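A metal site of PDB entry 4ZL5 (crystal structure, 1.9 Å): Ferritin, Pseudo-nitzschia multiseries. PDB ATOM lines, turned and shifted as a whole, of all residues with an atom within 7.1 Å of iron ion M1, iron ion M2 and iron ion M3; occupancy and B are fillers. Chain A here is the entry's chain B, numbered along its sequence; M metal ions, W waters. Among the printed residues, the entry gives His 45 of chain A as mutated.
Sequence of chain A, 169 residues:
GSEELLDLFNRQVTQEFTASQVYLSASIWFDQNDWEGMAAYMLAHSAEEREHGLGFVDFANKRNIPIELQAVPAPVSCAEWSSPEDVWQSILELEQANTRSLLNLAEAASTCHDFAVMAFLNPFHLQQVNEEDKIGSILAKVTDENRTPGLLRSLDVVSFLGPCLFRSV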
ATOM      1  N   GLN A  12       8.910 -10.629  14.293  1.00  0.00           N
ATOM      2  CA  GLN A  12       8.655  -9.674  15.366  1.00  0.00           C
ATOM      3  C   GLN A  12       7.534  -8.746  14.987  1.00  0.00           C
ATOM      4  O   GLN A  12       6.748  -8.363  15.817  1.00  0.00           O
ATOM      5  CB  GLN A  12       9.895  -8.856  15.662  1.00  0.00           C
ATOM      6  CG  GLN A  12       9.764  -7.983  16.878  1.00  0.00           C
ATOM      7  CD  GLN A  12       9.540  -8.796  18.153  1.00  0.00           C
ATOM      8  OE1 GLN A  12      10.030  -9.933  18.267  1.00  0.00           O
ATOM      9  NE2 GLN A  12       8.806  -8.242  19.069  1.00  0.00           N
ATOM     10  N   GLN A  15       4.410 -10.550  15.582  1.00  0.00           N
ATOM     11  CA  GLN A  15       4.159 -10.608  16.993  1.00  0.00           C
ATOM     12  C   GLN A  15       3.536  -9.292  17.484  1.00  0.00           C
ATOM     13  O   GLN A  15       2.652  -9.357  18.299  1.00  0.00           O
ATOM     14  CB  GLN A  15       5.458 -10.936  17.763  1.00  0.00           C
ATOM     15  CG  GLN A  15       5.362 -11.057  19.260  1.00  0.00           C
ATOM     16  CD  GLN A  15       4.389 -12.171  19.697  1.00  0.00           C
ATOM     17  OE1 GLN A  15       4.306 -13.224  19.006  1.00  0.00           O
ATOM     18  NE2 GLN A  15       3.616 -11.940  20.824  1.00  0.00           N
ATOM     19  N   GLU A  16       4.046  -8.159  17.022  1.00  0.00           N
ATOM     20  CA  GLU A  16       3.497  -6.876  17.471  1.00  0.00           C
ATOM     21  C   GLU A  16       2.080  -6.698  16.989  1.00  0.00           C
ATOM     22  O   GLU A  16       1.241  -6.265  17.772  1.00  0.00           O
ATOM     23  CB  GLU A  16       4.336  -5.708  16.946  1.00  0.00           C
ATOM     24  CG  GLU A  16       5.775  -5.691  17.386  1.00  0.00           C
ATOM     25  CD  GLU A  16       5.910  -5.580  18.906  1.00  0.00           C
ATOM     26  OE1 GLU A  16       4.987  -5.074  19.554  1.00  0.00           O
ATOM     27  OE2 GLU A  16       6.935  -6.059  19.426  1.00  0.00           O
ATOM     28  N   ALA A  19      -0.115  -9.050  18.996  1.00  0.00           N
ATOM     29  CA  ALA A  19      -0.407  -8.434  20.296  1.00  0.00           C
ATOM     30  C   ALA A  19      -1.415  -7.311  20.172  1.00  0.00           C
ATOM     31  O   ALA A  19      -2.315  -7.219  21.028  1.00  0.00           O
ATOM     32  CB  ALA A  19       0.871  -7.940  20.979  1.00  0.00           C
ATOM     33  N   TYR A  23      -4.804  -7.270  22.438  1.00  0.00           N
ATOM     34  CA  TYR A  23      -5.230  -6.150  23.253  1.00  0.00           C
ATOM     35  C   TYR A  23      -6.583  -5.647  22.821  1.00  0.00           C
ATOM     36  O   TYR A  23      -7.419  -5.273  23.669  1.00  0.00           O
ATOM     37  CB  TYR A  23      -4.203  -5.012  23.179  1.00  0.00           C
ATOM     38  CG  TYR A  23      -3.056  -5.112  24.128  1.00  0.00           C
ATOM     39  CD1 TYR A  23      -3.181  -4.754  25.444  1.00  0.00           C
ATOM     40  CD2 TYR A  23      -1.799  -5.507  23.715  1.00  0.00           C
ATOM     41  CE1 TYR A  23      -2.111  -4.795  26.323  1.00  0.00           C
ATOM     42  CE2 TYR A  23      -0.737  -5.626  24.620  1.00  0.00           C
ATOM     43  CZ  TYR A  23      -0.924  -5.235  25.915  1.00  0.00           C
ATOM     44  OH  TYR A  23       0.049  -5.206  26.845  1.00  0.00           O
ATOM     45  N   HIS A  45      -3.324   0.476  24.365  1.00  0.00           N
ATOM     46  CA  HIS A  45      -2.195  -0.327  24.302  1.00  0.00           C
ATOM     47  C   HIS A  45      -2.237  -1.104  22.941  1.00  0.00           C
ATOM     48  O   HIS A  45      -1.207  -1.331  22.371  1.00  0.00           O
ATOM     49  CB  HIS A  45      -2.095  -1.240  25.499  1.00  0.00           C
ATOM     50  CG  HIS A  45      -0.709  -1.698  25.771  1.00  0.00           C
ATOM     51  ND1 HIS A  45      -0.150  -1.724  27.030  1.00  0.00           N
ATOM     52  CD2 HIS A  45       0.267  -2.160  24.932  1.00  0.00           C
ATOM     53  CE1 HIS A  45       1.076  -2.227  26.968  1.00  0.00           C
ATOM     54  NE2 HIS A  45       1.369  -2.449  25.699  1.00  0.00           N
ATOM     55  N   GLU A  48      -0.675   1.124  20.516  1.00  0.00           N
ATOM     56  CA  GLU A  48       0.733   1.232  20.757  1.00  0.00           C
ATOM     57  C   GLU A  48       1.514  -0.010  20.259  1.00  0.00           C
ATOM     58  O   GLU A  48       2.652   0.125  19.705  1.00  0.00           O
ATOM     59  CB  GLU A  48       0.962   1.389  22.265  1.00  0.00           C
ATOM     60  CG  GLU A  48       2.408   1.149  22.671  1.00  0.00           C
ATOM     61  CD  GLU A  48       2.614   1.388  24.165  1.00  0.00           C
ATOM     62  OE1 GLU A  48       1.743   2.039  24.784  1.00  0.00           O
ATOM     63  OE2 GLU A  48       3.630   0.890  24.711  1.00  0.00           O
ATOM     64  N   GLU A  49       0.930  -1.182  20.406  1.00  0.00           N
ATOM     65  CA  GLU A  49       1.602  -2.367  19.772  1.00  0.00           C
ATOM     66  C   GLU A  49       1.702  -2.244  18.258  1.00  0.00           C
ATOM     67  O   GLU A  49       2.687  -2.656  17.627  1.00  0.00           O
ATOM     68  CB  GLU A  49       0.878  -3.625  20.047  1.00  0.00           C
ATOM     69  CG  GLU A  49       0.775  -4.014  21.458  1.00  0.00           C
ATOM     70  CD  GLU A  49       2.104  -4.285  22.132  1.00  0.00           C
ATOM     71  OE1 GLU A  49       3.139  -4.570  21.547  1.00  0.00           O
ATOM     72  OE2 GLU A  49       1.996  -4.305  23.304  1.00  0.00           O
ATOM     73  N   ARG A  50       0.622  -1.759  17.650  1.00  0.00           N
ATOM     74  CA  ARG A  50       0.627  -1.521  16.228  1.00  0.00           C
ATOM     75  C   ARG A  50       1.756  -0.538  15.906  1.00  0.00           C
ATOM     76  O   ARG A  50       2.501  -0.707  14.921  1.00  0.00           O
ATOM     77  CB  ARG A  50      -0.689  -0.952  15.720  1.00  0.00           C
ATOM     78  CG  ARG A  50      -0.688  -0.810  14.206  1.00  0.00           C
ATOM     79  CD  ARG A  50      -2.091  -0.802  13.568  1.00  0.00           C
ATOM     80  NE  ARG A  50      -2.024  -0.536  12.126  1.00  0.00           N
ATOM     81  CZ  ARG A  50      -1.835   0.693  11.647  1.00  0.00           C
ATOM     82  NH1 ARG A  50      -1.685   1.713  12.450  1.00  0.00           N
ATOM     83  NH2 ARG A  50      -1.652   0.889  10.365  1.00  0.00           N
ATOM     84  N   HIS A  52       4.598  -0.124  17.496  1.00  0.00           N
ATOM     85  CA  HIS A  52       5.841  -0.878  17.550  1.00  0.00           C
ATOM     86  C   HIS A  52       6.070  -1.671  16.256  1.00  0.00           C
ATOM     87  O   HIS A  52       7.183  -1.685  15.695  1.00  0.00           O
ATOM     88  CB  HIS A  52       5.898  -1.863  18.696  1.00  0.00           C
ATOM     89  CG  HIS A  52       5.720  -1.262  20.036  1.00  0.00           C
ATOM     90  ND1 HIS A  52       6.044   0.052  20.305  1.00  0.00           N
ATOM     91  CD2 HIS A  52       5.296  -1.810  21.199  1.00  0.00           C
ATOM     92  CE1 HIS A  52       5.779   0.298  21.570  1.00  0.00           C
ATOM     93  NE2 HIS A  52       5.328  -0.810  22.135  1.00  0.00           N
ATOM     94  N   GLY A  53       5.048  -2.370  15.810  1.00  0.00           N
ATOM     95  CA  GLY A  53       5.196  -3.072  14.548  1.00  0.00           C
ATOM     96  C   GLY A  53       5.600  -2.165  13.403  1.00  0.00           C
ATOM     97  O   GLY A  53       6.452  -2.535  12.594  1.00  0.00           O
ATOM     98  N   PHE A  56       9.261  -1.333  13.499  1.00  0.00           N
ATOM     99  CA  PHE A  56      10.015  -2.411  12.916  1.00  0.00           C
ATOM    100  C   PHE A  56       9.993  -2.448  11.427  1.00  0.00           C
ATOM    101  O   PHE A  56      11.045  -2.608  10.821  1.00  0.00           O
ATOM    102  CB  PHE A  56       9.620  -3.762  13.482  1.00  0.00           C
ATOM    103  CG  PHE A  56      10.245  -4.051  14.860  1.00  0.00           C
ATOM    104  CD1 PHE A  56       9.745  -3.440  16.003  1.00  0.00           C
ATOM    105  CD2 PHE A  56      11.320  -4.899  14.989  1.00  0.00           C
ATOM    106  CE1 PHE A  56      10.338  -3.625  17.248  1.00  0.00           C
ATOM    107  CE2 PHE A  56      11.924  -5.096  16.240  1.00  0.00           C
ATOM    108  CZ  PHE A  56      11.426  -4.461  17.363  1.00  0.00           C
ATOM    109  N   LEU A  94       1.190 -12.376  27.247  1.00  0.00           N
ATOM    110  CA  LEU A  94       1.449 -11.827  25.943  1.00  0.00           C
ATOM    111  C   LEU A  94       2.736 -10.970  25.920  1.00  0.00           C
ATOM    112  O   LEU A  94       3.613 -11.106  25.055  1.00  0.00           O
ATOM    113  CB  LEU A  94       0.222 -10.987  25.598  1.00  0.00           C
ATOM    114  CG  LEU A  94       0.270 -10.216  24.270  1.00  0.00           C
ATOM    115  CD1 LEU A  94       0.232 -11.191  23.157  1.00  0.00           C
ATOM    116  CD2 LEU A  94      -0.892  -9.247  24.117  1.00  0.00           C
ATOM    117  N   GLU A  95       2.833 -10.076  26.896  1.00  0.00           N
ATOM    118  CA  GLU A  95       4.023  -9.262  27.021  1.00  0.00           C
ATOM    119  C   GLU A  95       5.243 -10.045  27.358  1.00  0.00           C
ATOM    120  O   GLU A  95       6.329  -9.749  26.832  1.00  0.00           O
ATOM    121  CB  GLU A  95       3.822  -8.132  28.015  1.00  0.00           C
ATOM    122  CG  GLU A  95       2.882  -7.007  27.538  1.00  0.00           C
ATOM    123  CD  GLU A  95       3.359  -6.203  26.357  1.00  0.00           C
ATOM    124  OE1 GLU A  95       4.487  -6.340  25.841  1.00  0.00           O
ATOM    125  OE2 GLU A  95       2.554  -5.326  25.962  1.00  0.00           O
ATOM    126  N   ASN A  98       6.197 -11.273  24.090  1.00  0.00           N
ATOM    127  CA  ASN A  98       6.746 -10.157  23.291  1.00  0.00           C
ATOM    128  C   ASN A  98       8.257 -10.049  23.725  1.00  0.00           C
ATOM    129  O   ASN A  98       9.184 -10.013  22.881  1.00  0.00           O
ATOM    130  CB  ASN A  98       6.062  -8.764  23.491  1.00  0.00           C
ATOM    131  CG  ASN A  98       4.622  -8.590  22.855  1.00  0.00           C
ATOM    132  OD1 ASN A  98       4.157  -9.378  22.008  1.00  0.00           O
ATOM    133  ND2 ASN A  98       3.911  -7.502  23.306  1.00  0.00           N
ATOM    134  N   LEU A 102      11.750 -10.519  21.494  1.00  0.00           N
ATOM    135  CA  LEU A 102      12.791  -9.470  21.284  1.00  0.00           C
ATOM    136  C   LEU A 102      14.131  -9.924  21.648  1.00  0.00           C
ATOM    137  O   LEU A 102      15.124  -9.522  21.041  1.00  0.00           O
ATOM    138  CB  LEU A 102      12.554  -8.229  22.133  1.00  0.00           C
ATOM    139  CG  LEU A 102      11.480  -7.304  21.621  1.00  0.00           C
ATOM    140  CD1 LEU A 102      11.277  -6.243  22.703  1.00  0.00           C
ATOM    141  CD2 LEU A 102      11.863  -6.632  20.314  1.00  0.00           C
ATOM    142  N   PHE A 124      13.462  -0.739  22.886  1.00  0.00           N
ATOM    143  CA  PHE A 124      12.425  -1.740  23.054  1.00  0.00           C
ATOM    144  C   PHE A 124      12.726  -2.698  24.224  1.00  0.00           C
ATOM    145  O   PHE A 124      11.802  -3.073  24.966  1.00  0.00           O
ATOM    146  CB  PHE A 124      12.226  -2.534  21.764  1.00  0.00           C
ATOM    147  CG  PHE A 124      11.771  -1.702  20.597  1.00  0.00           C
ATOM    148  CD1 PHE A 124      10.400  -1.412  20.437  1.00  0.00           C
ATOM    149  CD2 PHE A 124      12.672  -1.196  19.667  1.00  0.00           C
ATOM    150  CE1 PHE A 124       9.959  -0.660  19.372  1.00  0.00           C
ATOM    151  CE2 PHE A 124      12.233  -0.464  18.566  1.00  0.00           C
ATOM    152  CZ  PHE A 124      10.889  -0.152  18.443  1.00  0.00           C
ATOM    153  N   GLN A 127      11.668  -0.683  27.135  1.00  0.00           N
ATOM    154  CA  GLN A 127      10.220  -0.484  27.199  1.00  0.00           C
ATOM    155  C   GLN A 127       9.546  -1.762  27.731  1.00  0.00           C
ATOM    156  O   GLN A 127       8.604  -1.653  28.551  1.00  0.00           O
ATOM    157  CB  GLN A 127       9.650  -0.176  25.823  1.00  0.00           C
ATOM    158  CG  GLN A 127       8.103  -0.150  25.814  1.00  0.00           C
ATOM    159  CD  GLN A 127       7.511   0.710  24.704  1.00  0.00           C
ATOM    160  OE1 GLN A 127       6.323   1.077  24.755  1.00  0.00           O
ATOM    161  NE2 GLN A 127       8.323   1.047  23.692  1.00  0.00           N
ATOM    162  N   GLN A 128      10.044  -2.914  27.319  1.00  0.00           N
ATOM    163  CA  GLN A 128       9.471  -4.214  27.716  1.00  0.00           C
ATOM    164  C   GLN A 128       9.627  -4.364  29.246  1.00  0.00           C
ATOM    165  O   GLN A 128       8.670  -4.816  29.914  1.00  0.00           O
ATOM    166  CB  GLN A 128      10.051  -5.428  26.995  1.00  0.00           C
ATOM    167  CG  GLN A 128       9.511  -5.608  25.585  1.00  0.00           C
ATOM    168  CD  GLN A 128       7.987  -5.581  25.569  1.00  0.00           C
ATOM    169  OE1 GLN A 128       7.365  -4.563  25.197  1.00  0.00           O
ATOM    170  NE2 GLN A 128       7.386  -6.613  26.164  1.00  0.00           N
ATOM    171  N   GLU A 131       6.881  -2.207  30.696  1.00  0.00           N
ATOM    172  CA  GLU A 131       5.555  -2.795  30.468  1.00  0.00           C
ATOM    173  C   GLU A 131       5.255  -3.980  31.313  1.00  0.00           C
ATOM    174  O   GLU A 131       4.177  -4.029  31.888  1.00  0.00           O
ATOM    175  CB  GLU A 131       5.356  -3.167  28.976  1.00  0.00           C
ATOM    176  CG  GLU A 131       5.214  -1.876  28.214  1.00  0.00           C
ATOM    177  CD  GLU A 131       4.833  -2.062  26.736  1.00  0.00           C
ATOM    178  OE1 GLU A 131       4.402  -3.165  26.423  1.00  0.00           O
ATOM    179  OE2 GLU A 131       5.054  -1.121  25.941  1.00  0.00           O
ATOM    180  N   ILE A 135       2.130  -4.025  33.952  1.00  0.00           N
ATOM    181  CA  ILE A 135       1.015  -4.978  33.812  1.00  0.00           C
ATOM    182  C   ILE A 135       1.032  -5.977  34.995  1.00  0.00           C
ATOM    183  O   ILE A 135      -0.004  -6.376  35.516  1.00  0.00           O
ATOM    184  CB  ILE A 135       1.093  -5.708  32.456  1.00  0.00           C
ATOM    185  CG1 ILE A 135       0.988  -4.701  31.320  1.00  0.00           C
ATOM    186  CG2 ILE A 135       0.051  -6.793  32.354  1.00  0.00           C
ATOM    187  CD1 ILE A 135       1.502  -5.252  30.014  1.00  0.00           C
HETATM  188 FE    FE M   1       3.231  -3.600  24.815  1.00  0.00          FE
HETATM  189 FE    FE M   2       5.465  -0.964  24.152  1.00  0.00          FE
HETATM  190 FE    FE M   3       5.097  -4.592  21.725  1.00  0.00          FE
HETATM  191  O   HOH W   1       3.434  -1.801  24.002  1.00  0.00           O
HETATM  192  O   HOH W   2       7.412  -4.648  21.727  1.00  0.00           O
HETATM  193  O   HOH W   3       5.051  -4.537  24.020  1.00  0.00           O
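The side-chain carboxylate (OE1) of Glu 131 sits close to the side-chain amide oxygen (OE1) of Gln 128, 3.5 Å away.
A ring nitrogen (ND1) of His 52 sits close to the backbone carbonyl oxygen (O) of Glu 48 (3.4 Å).
The side-chain carboxylate (OE2) of Glu 95 lies close to the side-chain hydroxyl (OH) of Tyr 23 (2.7 Å).
OE1 of Glu 95 sits at hydrogen-bond distance from NE2 of Gln 128 (2.9 Å).
The side-chain amide nitrogen (NE2) of Gln 12 lies within hydrogen-bond range of the side-chain carboxylate (OE2) of Glu 16.
The side-chain amide oxygen (OE1) of Gln 127 lies close to the side-chain carboxylate (OE2) of Glu 48, at 2.7 Å.
A ring nitrogen (ND1) of His 45 lies close to the side-chain hydroxyl (OH) of Tyr 23, 3.5 Å away.
OD1 of Asn 98 sits at hydrogen-bond distance from NE2 of Gln 15 (2.9 Å).
Four residues have an atom within 4 Å of iron ion M1: His 45, Glu 49, Glu 95 and Glu 131.
The nearest printed residue that does not touch iron ion M1 is Tyr 23 (4.1 Å).
Four residues have an atom within 4 Å of iron ion M2: Glu 48, His 52, Gln 127 and Glu 131.
The nearest printed residue that does not touch iron ion M2 is Gln 128 (4.2 Å).
Residues that only touch iron ion M3: Asn 98.
Within 4 Å of iron ion M3: Glu 16, Glu 49, His 52 and Asn 98.
Iron ion M1 is bound by water W1, at 2.0 Å.
Iron ion M1 is bound by OE1 of Glu 131 (2.0 Å).
Iron ion M1 is bound by OE2 of Glu 49.
OE2 of Glu 95 is bound to iron ion M1.
Water W3 is bound to iron ion M1.
NE2 of His 45 binds iron ion M1, 2.4 Å away.
Iron ion M1 has six donor atoms within binding distance.
Iron ion M2 is bound by the side-chain carboxylate of Glu 131, a ring nitrogen (NE2) of His 52, water W1 and the side-chain amide oxygen of Gln 127.
Iron ion M2 has four donor atoms within binding distance.
Slightly farther from iron ion M2 lies the side-chain carboxylate (OE2) of Glu 48 (2.7 Å).
Iron ion M3 is bound by OE1 of Glu 49, at 2.0 Å.
Iron ion M3 is bound by OE1 of Glu 16, at 2.2 Å.
Iron ion M3 is bound by water W3.
Iron ion M3 is bound by water W2 (2.3 Å).
Water W3 lies within hydrogen-bond range of the side-chain amide oxygen (OE1) of Gln 128 (2.6 Å), the side-chain carboxylate (OE1) of Glu 95 (2.6 Å) and the side-chain amide nitrogen (ND2) of Asn 98 (3.3 Å).
Water W2 lies within hydrogen-bond range of the side-chain carboxylate of Glu 16 (2.7 Å) and the side-chain amide oxygen of Gln 128 (3.5 Å).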
